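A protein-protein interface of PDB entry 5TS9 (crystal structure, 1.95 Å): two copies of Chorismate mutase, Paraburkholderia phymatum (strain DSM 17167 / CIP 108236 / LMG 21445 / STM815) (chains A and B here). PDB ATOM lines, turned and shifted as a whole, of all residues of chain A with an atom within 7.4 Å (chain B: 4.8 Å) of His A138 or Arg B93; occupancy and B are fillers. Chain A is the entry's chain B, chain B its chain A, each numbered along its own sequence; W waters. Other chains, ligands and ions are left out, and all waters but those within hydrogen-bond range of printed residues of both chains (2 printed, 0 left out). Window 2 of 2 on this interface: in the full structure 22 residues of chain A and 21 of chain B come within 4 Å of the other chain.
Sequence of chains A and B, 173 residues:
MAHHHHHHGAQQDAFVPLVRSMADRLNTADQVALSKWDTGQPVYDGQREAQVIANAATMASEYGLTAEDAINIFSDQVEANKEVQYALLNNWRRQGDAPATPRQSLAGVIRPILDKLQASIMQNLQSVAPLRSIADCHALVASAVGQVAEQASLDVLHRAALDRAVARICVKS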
ATOM      1  N   ASP A  13     -21.414 -32.747  -2.649  1.00  0.00           N
ATOM      2  CA  ASP A  13     -21.112 -31.612  -1.782  1.00  0.00           C
ATOM      3  C   ASP A  13     -19.656 -31.791  -1.372  1.00  0.00           C
ATOM      4  O   ASP A  13     -19.345 -32.689  -0.585  1.00  0.00           O
ATOM      5  CB  ASP A  13     -22.053 -31.595  -0.579  1.00  0.00           C
ATOM      6  CG  ASP A  13     -21.795 -30.443   0.367  1.00  0.00           C
ATOM      7  OD1 ASP A  13     -20.637 -29.964   0.489  1.00  0.00           O
ATOM      8  OD2 ASP A  13     -22.781 -30.042   1.044  1.00  0.00           O
ATOM      9  N   PHE A  15     -17.695 -30.632   0.663  1.00  0.00           N
ATOM     10  CA  PHE A  15     -17.278 -30.599   2.057  1.00  0.00           C
ATOM     11  C   PHE A  15     -17.693 -31.823   2.868  1.00  0.00           C
ATOM     12  O   PHE A  15     -17.410 -31.864   4.067  1.00  0.00           O
ATOM     13  CB  PHE A  15     -17.795 -29.323   2.730  1.00  0.00           C
ATOM     14  CG  PHE A  15     -17.123 -28.069   2.221  1.00  0.00           C
ATOM     15  CD1 PHE A  15     -15.884 -27.676   2.720  1.00  0.00           C
ATOM     16  CD2 PHE A  15     -17.708 -27.304   1.222  1.00  0.00           C
ATOM     17  CE1 PHE A  15     -15.250 -26.536   2.238  1.00  0.00           C
ATOM     18  CE2 PHE A  15     -17.069 -26.150   0.731  1.00  0.00           C
ATOM     19  CZ  PHE A  15     -15.848 -25.772   1.240  1.00  0.00           C
ATOM     20  N   LEU A 131     -11.990 -23.990  -2.224  1.00  0.00           N
ATOM     21  CA  LEU A 131     -13.421 -23.817  -2.047  1.00  0.00           C
ATOM     22  C   LEU A 131     -13.785 -23.159  -0.733  1.00  0.00           C
ATOM     23  O   LEU A 131     -14.951 -22.819  -0.547  1.00  0.00           O
ATOM     24  CB  LEU A 131     -14.142 -25.168  -2.152  1.00  0.00           C
ATOM     25  CG  LEU A 131     -13.858 -25.956  -3.433  1.00  0.00           C
ATOM     26  CD1 LEU A 131     -14.405 -27.366  -3.317  1.00  0.00           C
ATOM     27  CD2 LEU A 131     -14.499 -25.267  -4.626  1.00  0.00           C
ATOM     28  N   ARG A 132     -12.830 -22.971   0.182  1.00  0.00           N
ATOM     29  CA  ARG A 132     -13.188 -22.480   1.512  1.00  0.00           C
ATOM     30  C   ARG A 132     -13.568 -21.018   1.513  1.00  0.00           C
ATOM     31  O   ARG A 132     -14.070 -20.520   2.528  1.00  0.00           O
ATOM     32  CB  ARG A 132     -12.041 -22.725   2.492  1.00  0.00           C
ATOM     33  CG  ARG A 132     -11.853 -24.207   2.772  1.00  0.00           C
ATOM     34  CD  ARG A 132     -10.665 -24.498   3.701  1.00  0.00           C
ATOM     35  NE  ARG A 132     -10.866 -23.841   4.982  1.00  0.00           N
ATOM     36  CZ  ARG A 132      -9.914 -23.655   5.885  1.00  0.00           C
ATOM     37  NH1 ARG A 132      -8.672 -24.074   5.641  1.00  0.00           N
ATOM     38  NH2 ARG A 132     -10.209 -23.033   7.023  1.00  0.00           N
ATOM     39  N   ILE A 134     -15.330 -19.584  -1.293  1.00  0.00           N
ATOM     40  CA  ILE A 134     -16.385 -19.314  -2.268  1.00  0.00           C
ATOM     41  C   ILE A 134     -17.673 -18.931  -1.542  1.00  0.00           C
ATOM     42  O   ILE A 134     -17.913 -19.307  -0.386  1.00  0.00           O
ATOM     43  CB  ILE A 134     -16.623 -20.502  -3.227  1.00  0.00           C
ATOM     44  CG1 ILE A 134     -17.360 -21.662  -2.529  1.00  0.00           C
ATOM     45  CG2 ILE A 134     -15.310 -20.963  -3.882  1.00  0.00           C
ATOM     46  CD1 ILE A 134     -17.909 -22.738  -3.487  1.00  0.00           C
ATOM     47  N   ALA A 135     -18.528 -18.193  -2.258  1.00  0.00           N
ATOM     48  CA  ALA A 135     -19.696 -17.566  -1.635  1.00  0.00           C
ATOM     49  C   ALA A 135     -20.637 -18.595  -1.025  1.00  0.00           C
ATOM     50  O   ALA A 135     -21.194 -18.373   0.054  1.00  0.00           O
ATOM     51  CB  ALA A 135     -20.445 -16.715  -2.660  1.00  0.00           C
ATOM     52  N   ASP A 136     -20.827 -19.724  -1.693  1.00  0.00           N
ATOM     53  CA  ASP A 136     -21.764 -20.717  -1.188  1.00  0.00           C
ATOM     54  C   ASP A 136     -21.168 -21.629  -0.129  1.00  0.00           C
ATOM     55  O   ASP A 136     -21.785 -22.649   0.181  1.00  0.00           O
ATOM     56  CB  ASP A 136     -22.302 -21.560  -2.345  1.00  0.00           C
ATOM     57  CG  ASP A 136     -23.201 -20.757  -3.278  1.00  0.00           C
ATOM     58  OD1 ASP A 136     -23.912 -19.841  -2.783  1.00  0.00           O
ATOM     59  OD2 ASP A 136     -23.181 -21.040  -4.501  1.00  0.00           O
ATOM     60  N   CYS A 137     -19.999 -21.309   0.431  1.00  0.00           N
ATOM     61  CA  CYS A 137     -19.353 -22.261   1.339  1.00  0.00           C
ATOM     62  C   CYS A 137     -20.235 -22.569   2.553  1.00  0.00           C
ATOM     63  O   CYS A 137     -20.343 -23.728   2.966  1.00  0.00           O
ATOM     64  CB  CYS A 137     -17.971 -21.738   1.774  1.00  0.00           C
ATOM     65  SG  CYS A 137     -17.074 -22.824   2.962  1.00  0.00           S
ATOM     66  N   HIS A 138     -20.870 -21.552   3.145  1.00  0.00           N
ATOM     67  CA  HIS A 138     -21.659 -21.786   4.354  1.00  0.00           C
ATOM     68  C   HIS A 138     -22.779 -22.792   4.090  1.00  0.00           C
ATOM     69  O   HIS A 138     -22.975 -23.751   4.852  1.00  0.00           O
ATOM     70  CB  HIS A 138     -22.267 -20.474   4.858  1.00  0.00           C
ATOM     71  CG  HIS A 138     -21.325 -19.609   5.629  1.00  0.00           C
ATOM     72  ND1 HIS A 138     -20.579 -20.073   6.690  1.00  0.00           N
ATOM     73  CD2 HIS A 138     -21.049 -18.289   5.525  1.00  0.00           C
ATOM     74  CE1 HIS A 138     -19.857 -19.084   7.188  1.00  0.00           C
ATOM     75  NE2 HIS A 138     -20.133 -17.987   6.506  1.00  0.00           N
ATOM     76  N   ALA A 139     -23.537 -22.565   3.018  1.00  0.00           N
ATOM     77  CA  ALA A 139     -24.607 -23.469   2.625  1.00  0.00           C
ATOM     78  C   ALA A 139     -24.090 -24.884   2.381  1.00  0.00           C
ATOM     79  O   ALA A 139     -24.725 -25.859   2.785  1.00  0.00           O
ATOM     80  CB  ALA A 139     -25.292 -22.927   1.369  1.00  0.00           C
ATOM     81  N   LEU A 140     -22.958 -25.026   1.689  1.00  0.00           N
ATOM     82  CA  LEU A 140     -22.458 -26.368   1.410  1.00  0.00           C
ATOM     83  C   LEU A 140     -22.074 -27.085   2.704  1.00  0.00           C
ATOM     84  O   LEU A 140     -22.326 -28.286   2.870  1.00  0.00           O
ATOM     85  CB  LEU A 140     -21.256 -26.292   0.468  1.00  0.00           C
ATOM     86  CG  LEU A 140     -21.456 -25.767  -0.957  1.00  0.00           C
ATOM     87  CD1 LEU A 140     -20.103 -25.485  -1.634  1.00  0.00           C
ATOM     88  CD2 LEU A 140     -22.236 -26.790  -1.749  1.00  0.00           C
ATOM     89  N   VAL A 141     -21.462 -26.360   3.629  1.00  0.00           N
ATOM     90  CA  VAL A 141     -21.011 -26.979   4.869  1.00  0.00           C
ATOM     91  C   VAL A 141     -22.214 -27.372   5.711  1.00  0.00           C
ATOM     92  O   VAL A 141     -22.275 -28.486   6.239  1.00  0.00           O
ATOM     93  CB  VAL A 141     -20.039 -26.032   5.608  1.00  0.00           C
ATOM     94  CG1 VAL A 141     -19.836 -26.438   7.102  1.00  0.00           C
ATOM     95  CG2 VAL A 141     -18.664 -25.968   4.865  1.00  0.00           C
ATOM     96  N   ALA A 142     -23.228 -26.501   5.769  1.00  0.00           N
ATOM     97  CA  ALA A 142     -24.434 -26.793   6.541  1.00  0.00           C
ATOM     98  C   ALA A 142     -25.123 -28.044   6.011  1.00  0.00           C
ATOM     99  O   ALA A 142     -25.566 -28.907   6.781  1.00  0.00           O
ATOM    100  CB  ALA A 142     -25.396 -25.598   6.476  1.00  0.00           C
ATOM    101  N   SER A 143     -25.236 -28.148   4.686  1.00  0.00           N
ATOM    102  CA  SER A 143     -25.885 -29.312   4.099  1.00  0.00           C
ATOM    103  C   SER A 143     -25.058 -30.562   4.346  1.00  0.00           C
ATOM    104  O   SER A 143     -25.609 -31.652   4.524  1.00  0.00           O
ATOM    105  CB  SER A 143     -26.096 -29.099   2.601  1.00  0.00           C
ATOM    106  OG  SER A 143     -26.769 -30.201   2.034  1.00  0.00           O
ATOM    107  N   ALA A 144     -23.739 -30.413   4.350  1.00  0.00           N
ATOM    108  CA  ALA A 144     -22.848 -31.523   4.668  1.00  0.00           C
ATOM    109  C   ALA A 144     -23.071 -32.012   6.090  1.00  0.00           C
ATOM    110  O   ALA A 144     -23.122 -33.226   6.326  1.00  0.00           O
ATOM    111  CB  ALA A 144     -21.389 -31.098   4.464  1.00  0.00           C
ATOM    112  N   ASP A 163     -22.091 -28.801  14.216  1.00  0.00           N
ATOM    113  CA  ASP A 163     -22.167 -27.428  13.701  1.00  0.00           C
ATOM    114  C   ASP A 163     -21.108 -26.532  14.343  1.00  0.00           C
ATOM    115  O   ASP A 163     -20.607 -25.591  13.702  1.00  0.00           O
ATOM    116  CB  ASP A 163     -23.549 -26.827  13.948  1.00  0.00           C
ATOM    117  CG  ASP A 163     -24.609 -27.323  12.943  1.00  0.00           C
ATOM    118  OD1 ASP A 163     -24.252 -27.548  11.762  1.00  0.00           O
ATOM    119  OD2 ASP A 163     -25.801 -27.446  13.328  1.00  0.00           O
ATOM    120  N   VAL A 166     -17.465 -27.364  12.610  1.00  0.00           N
ATOM    121  CA  VAL A 166     -17.289 -26.875  11.236  1.00  0.00           C
ATOM    122  C   VAL A 166     -17.291 -25.348  11.155  1.00  0.00           C
ATOM    123  O   VAL A 166     -17.250 -24.774  10.056  1.00  0.00           O
ATOM    124  CB  VAL A 166     -18.387 -27.441  10.304  1.00  0.00           C
ATOM    125  CG1 VAL A 166     -18.435 -28.971  10.348  1.00  0.00           C
ATOM    126  CG2 VAL A 166     -19.760 -26.812  10.642  1.00  0.00           C
ATOM    127  N   ALA A 167     -17.285 -24.685  12.314  1.00  0.00           N
ATOM    128  CA  ALA A 167     -17.484 -23.234  12.399  1.00  0.00           C
ATOM    129  C   ALA A 167     -16.599 -22.419  11.450  1.00  0.00           C
ATOM    130  O   ALA A 167     -17.033 -21.384  10.919  1.00  0.00           O
ATOM    131  CB  ALA A 167     -17.229 -22.781  13.837  1.00  0.00           C
ATOM    132  N   ARG A 168     -15.341 -22.812  11.264  1.00  0.00           N
ATOM    133  CA  ARG A 168     -14.448 -21.907  10.539  1.00  0.00           C
ATOM    134  C   ARG A 168     -13.803 -22.598   9.353  1.00  0.00           C
ATOM    135  O   ARG A 168     -12.688 -22.253   8.935  1.00  0.00           O
ATOM    136  CB  ARG A 168     -13.408 -21.307  11.481  1.00  0.00           C
ATOM    137  CG  ARG A 168     -14.075 -20.333  12.461  1.00  0.00           C
ATOM    138  CD  ARG A 168     -13.065 -19.637  13.329  1.00  0.00           C
ATOM    139  NE  ARG A 168     -12.553 -20.467  14.427  1.00  0.00           N
ATOM    140  CZ  ARG A 168     -11.782 -19.971  15.390  1.00  0.00           C
ATOM    141  NH1 ARG A 168     -11.463 -18.673  15.357  1.00  0.00           N
ATOM    142  NH2 ARG A 168     -11.352 -20.743  16.379  1.00  0.00           N
ATOM    143  N   ILE A 169     -14.501 -23.589   8.809  1.00  0.00           N
ATOM    144  CA  ILE A 169     -14.148 -24.087   7.494  1.00  0.00           C
ATOM    145  C   ILE A 169     -14.233 -22.962   6.473  1.00  0.00           C
ATOM    146  O   ILE A 169     -13.298 -22.729   5.697  1.00  0.00           O
ATOM    147  CB  ILE A 169     -15.047 -25.281   7.126  1.00  0.00           C
ATOM    148  CG1 ILE A 169     -14.832 -26.423   8.151  1.00  0.00           C
ATOM    149  CG2 ILE A 169     -14.775 -25.725   5.659  1.00  0.00           C
ATOM    150  CD1 ILE A 169     -15.667 -27.703   7.860  1.00  0.00           C
ATOM    151  N   CYS A 170     -15.342 -22.230   6.468  1.00  0.00           N
ATOM    152  CA  CYS A 170     -15.501 -21.149   5.510  1.00  0.00           C
ATOM    153  C   CYS A 170     -14.763 -19.919   6.015  1.00  0.00           C
ATOM    154  O   CYS A 170     -14.953 -19.497   7.162  1.00  0.00           O
ATOM    155  CB  CYS A 170     -16.976 -20.830   5.285  1.00  0.00           C
ATOM    156  SG  CYS A 170     -17.917 -22.294   4.776  1.00  0.00           S
ATOM    157  N   VAL A 171     -13.901 -19.355   5.174  1.00  0.00           N
ATOM    158  CA  VAL A 171     -13.105 -18.192   5.559  1.00  0.00           C
ATOM    159  C   VAL A 171     -13.235 -17.156   4.451  1.00  0.00           C
ATOM    160  O   VAL A 171     -13.083 -17.486   3.270  1.00  0.00           O
ATOM    161  CB  VAL A 171     -11.629 -18.555   5.834  1.00  0.00           C
ATOM    162  CG1 VAL A 171     -11.521 -19.585   6.969  1.00  0.00           C
ATOM    163  CG2 VAL A 171     -10.962 -19.090   4.593  1.00  0.00           C
ATOM    164  N   LYS A 172     -13.558 -15.920   4.831  1.00  0.00           N
ATOM    165  CA  LYS A 172     -13.906 -14.849   3.887  1.00  0.00           C
ATOM    166  C   LYS A 172     -12.859 -14.624   2.801  1.00  0.00           C
ATOM    167  O   LYS A 172     -11.656 -14.741   3.052  1.00  0.00           O
ATOM    168  CB  LYS A 172     -14.136 -13.542   4.649  1.00  0.00           C
ATOM    169  N   TRP B  37     -27.925 -13.631  11.173  1.00  0.00           N
ATOM    170  CA  TRP B  37     -28.568 -14.150   9.973  1.00  0.00           C
ATOM    171  C   TRP B  37     -28.957 -13.014   9.023  1.00  0.00           C
ATOM    172  O   TRP B  37     -28.761 -13.120   7.807  1.00  0.00           O
ATOM    173  CB  TRP B  37     -29.799 -14.986  10.367  1.00  0.00           C
ATOM    174  CG  TRP B  37     -30.687 -15.419   9.191  1.00  0.00           C
ATOM    175  CD1 TRP B  37     -31.730 -14.720   8.632  1.00  0.00           C
ATOM    176  CD2 TRP B  37     -30.597 -16.649   8.463  1.00  0.00           C
ATOM    177  NE1 TRP B  37     -32.283 -15.445   7.594  1.00  0.00           N
ATOM    178  CE2 TRP B  37     -31.601 -16.629   7.471  1.00  0.00           C
ATOM    179  CE3 TRP B  37     -29.752 -17.767   8.551  1.00  0.00           C
ATOM    180  CZ2 TRP B  37     -31.796 -17.691   6.581  1.00  0.00           C
ATOM    181  CZ3 TRP B  37     -29.951 -18.819   7.671  1.00  0.00           C
ATOM    182  CH2 TRP B  37     -30.959 -18.769   6.691  1.00  0.00           C
ATOM    183  N   LEU B  89     -27.930 -21.079  13.417  1.00  0.00           N
ATOM    184  CA  LEU B  89     -27.648 -20.568  12.080  1.00  0.00           C
ATOM    185  C   LEU B  89     -27.576 -21.695  11.072  1.00  0.00           C
ATOM    186  O   LEU B  89     -28.084 -21.570   9.953  1.00  0.00           O
ATOM    187  CB  LEU B  89     -26.346 -19.778  12.087  1.00  0.00           C
ATOM    188  CG  LEU B  89     -26.488 -18.399  12.704  1.00  0.00           C
ATOM    189  CD1 LEU B  89     -25.123 -17.860  12.968  1.00  0.00           C
ATOM    190  CD2 LEU B  89     -27.320 -17.451  11.775  1.00  0.00           C
ATOM    191  N   ASN B  90     -26.954 -22.820  11.446  1.00  0.00           N
ATOM    192  CA  ASN B  90     -26.885 -23.909  10.477  1.00  0.00           C
ATOM    193  C   ASN B  90     -28.220 -24.616  10.345  1.00  0.00           C
ATOM    194  O   ASN B  90     -28.532 -25.119   9.260  1.00  0.00           O
ATOM    195  CB  ASN B  90     -25.775 -24.901  10.838  1.00  0.00           C
ATOM    196  CG  ASN B  90     -24.468 -24.606  10.096  1.00  0.00           C
ATOM    197  OD1 ASN B  90     -24.385 -23.636   9.339  1.00  0.00           O
ATOM    198  ND2 ASN B  90     -23.443 -25.454  10.300  1.00  0.00           N
ATOM    199  N   ASN B  91     -29.015 -24.676  11.421  1.00  0.00           N
ATOM    200  CA  ASN B  91     -30.380 -25.179  11.289  1.00  0.00           C
ATOM    201  C   ASN B  91     -31.149 -24.351  10.272  1.00  0.00           C
ATOM    202  O   ASN B  91     -31.825 -24.895   9.398  1.00  0.00           O
ATOM    203  CB  ASN B  91     -31.113 -25.156  12.635  1.00  0.00           C
ATOM    204  CG  ASN B  91     -30.643 -26.247  13.565  1.00  0.00           C
ATOM    205  OD1 ASN B  91     -29.870 -27.098  13.155  1.00  0.00           O
ATOM    206  ND2 ASN B  91     -31.106 -26.227  14.815  1.00  0.00           N
ATOM    207  N   TRP B  92     -31.049 -23.031  10.378  1.00  0.00           N
ATOM    208  CA  TRP B  92     -31.755 -22.147   9.443  1.00  0.00           C
ATOM    209  C   TRP B  92     -31.177 -22.258   8.043  1.00  0.00           C
ATOM    210  O   TRP B  92     -31.923 -22.255   7.055  1.00  0.00           O
ATOM    211  CB  TRP B  92     -31.671 -20.708   9.942  1.00  0.00           C
ATOM    212  CG  TRP B  92     -32.280 -20.554  11.286  1.00  0.00           C
ATOM    213  CD1 TRP B  92     -33.210 -21.385  11.867  1.00  0.00           C
ATOM    214  CD2 TRP B  92     -32.008 -19.518  12.236  1.00  0.00           C
ATOM    215  NE1 TRP B  92     -33.531 -20.919  13.134  1.00  0.00           N
ATOM    216  CE2 TRP B  92     -32.804 -19.776  13.378  1.00  0.00           C
ATOM    217  CE3 TRP B  92     -31.166 -18.404  12.235  1.00  0.00           C
ATOM    218  CZ2 TRP B  92     -32.783 -18.948  14.515  1.00  0.00           C
ATOM    219  CZ3 TRP B  92     -31.144 -17.578  13.356  1.00  0.00           C
ATOM    220  CH2 TRP B  92     -31.949 -17.860  14.486  1.00  0.00           C
ATOM    221  N   ARG B  93     -29.851 -22.362   7.936  1.00  0.00           N
ATOM    222  CA  ARG B  93     -29.233 -22.534   6.618  1.00  0.00           C
ATOM    223  C   ARG B  93     -29.765 -23.780   5.914  1.00  0.00           C
ATOM    224  O   ARG B  93     -29.998 -23.758   4.702  1.00  0.00           O
ATOM    225  CB  ARG B  93     -27.702 -22.597   6.740  1.00  0.00           C
ATOM    226  CG  ARG B  93     -27.019 -21.254   6.990  1.00  0.00           C
ATOM    227  CD  ARG B  93     -25.513 -21.360   6.838  1.00  0.00           C
ATOM    228  NE  ARG B  93     -24.846 -20.108   7.178  1.00  0.00           N
ATOM    229  CZ  ARG B  93     -24.227 -19.871   8.326  1.00  0.00           C
ATOM    230  NH1 ARG B  93     -24.157 -20.817   9.262  1.00  0.00           N
ATOM    231  NH2 ARG B  93     -23.663 -18.685   8.532  1.00  0.00           N
ATOM    232  N   ARG B  94     -29.985 -24.873   6.661  1.00  0.00           N
ATOM    233  CA  ARG B  94     -30.460 -26.109   6.035  1.00  0.00           C
ATOM    234  C   ARG B  94     -31.920 -26.002   5.598  1.00  0.00           C
ATOM    235  O   ARG B  94     -32.342 -26.709   4.675  1.00  0.00           O
ATOM    236  CB  ARG B  94     -30.287 -27.296   6.996  1.00  0.00           C
ATOM    237  CG  ARG B  94     -28.832 -27.782   7.156  1.00  0.00           C
ATOM    238  CD  ARG B  94     -28.701 -29.015   8.097  1.00  0.00           C
ATOM    239  NE  ARG B  94     -28.715 -28.634   9.510  1.00  0.00           N
ATOM    240  CZ  ARG B  94     -27.642 -28.306  10.227  1.00  0.00           C
ATOM    241  NH1 ARG B  94     -26.417 -28.332   9.690  1.00  0.00           N
ATOM    242  NH2 ARG B  94     -27.789 -27.977  11.509  1.00  0.00           N
ATOM    243  N   GLN B  95     -32.710 -25.154   6.249  1.00  0.00           N
ATOM    244  CA  GLN B  95     -34.110 -24.976   5.851  1.00  0.00           C
ATOM    245  C   GLN B  95     -34.295 -23.863   4.832  1.00  0.00           C
ATOM    246  O   GLN B  95     -35.295 -23.869   4.099  1.00  0.00           O
ATOM    247  CB  GLN B  95     -34.981 -24.687   7.084  1.00  0.00           C
ATOM    248  CG  GLN B  95     -35.099 -25.863   8.046  1.00  0.00           C
ATOM    249  CD  GLN B  95     -35.344 -25.440   9.496  1.00  0.00           C
ATOM    250  OE1 GLN B  95     -35.773 -24.315   9.765  1.00  0.00           O
ATOM    251  NE2 GLN B  95     -35.063 -26.344  10.437  1.00  0.00           N
ATOM    252  N   GLY B  96     -33.358 -22.919   4.754  1.00  0.00           N
ATOM    253  CA  GLY B  96     -33.478 -21.817   3.819  1.00  0.00           C
ATOM    254  C   GLY B  96     -34.072 -20.548   4.378  1.00  0.00           C
ATOM    255  O   GLY B  96     -34.202 -19.566   3.631  1.00  0.00           O
HETATM  256  O   HOH W   1     -27.875 -28.084  14.837  1.00  0.00           O
HETATM  257  O   HOH W   2     -21.188 -23.723  11.684  1.00  0.00           O
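OD1 of Asn B90 sits at hydrogen-bond distance from NH1 of Arg B93 (2.8 Å). The side-chain amide oxygen (OD1) of Asn B91 lies within hydrogen-bond range of the guanidinium group (NH2) of Arg B94 (2.8 Å). The backbone NH (N) of His A138 lies within hydrogen-bond range of the side-chain sulfur (SG) of Cys A170, at 3.5 Å. The side-chain sulfur (SG) of Cys A137 is disulfide-bonded to the side-chain sulfur (SG) of Cys A170.
Of the printed residues of chain B, His A138 touches Arg B93 (3.5 Å). Of the printed residues of chain A, Arg B93 touches His A138 (3.5 Å) and Ala A142 (3.8 Å). Printed residues of chain B within 4 Å of Asp A163: Asn B90 and Arg B94. Of the printed residues of chain A, Arg B94 touches Ala A142 (3.1 Å) and Asp A163 (2.7 Å). Of the printed residues of chain B, Ala A142 touches Asn B90 (3.6 Å), Arg B93 (3.8 Å) and Arg B94 (3.1 Å). Of the printed residues of chain A, Asn B90 touches Ala A142, Asp A163 and Val A166. Asp A136 touches none of the printed residues of chain B. The nearest residue of chain B that does not touch His A138 is Asn B90 (4.7 Å). The nearest residue of chain A that does not touch Arg B93 is Ala A139 (4.5 Å). The nearest printed residue of chain A that does not touch Asn B90 is His A138 (4.7 Å).
The side-chain carboxylate of Asp A163 sits at hydrogen-bond distance from the side-chain amide nitrogen of Asn B90 (2.7 Å). The guanidinium group (NH1) of Arg B94 lies within hydrogen-bond range of the backbone carbonyl oxygen (O) of Ala A142 (3.1 Å). OD2 of Asp A163 is in salt-bridge range of NH2 of Arg B94 (2.7 Å).
Hydrophobic or aromatic side chains of chain A that line the printed part of chain B: His A138, Ala A142 and Val A166. Among the printed residues, Asp or Glu carboxylates within 4 Å of a Lys or Arg side-chain nitrogen of the other chain: Asp A163 with Arg B94 (2.7 Å).
No position is printed for both chains.
Among the printed residues, pairs that only touch across the chains: His A138 with Arg B93, Ala A142 with Asn B90, Ala A142 with Arg B93 and Val A166 with Asn B90.
Water W1 lies within hydrogen-bond range of the side-chain carboxylate (OD2) of Asp A163 (2.6 Å), the side-chain amide oxygen (OD1) of Asn B91 (2.8 Å) and the guanidinium group (NH2) of Arg B94 (3.3 Å). Water W2 lies within hydrogen-bond range of O of Asp A163 (2.8 Å) and ND2 of Asn B90 (3.2 Å).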
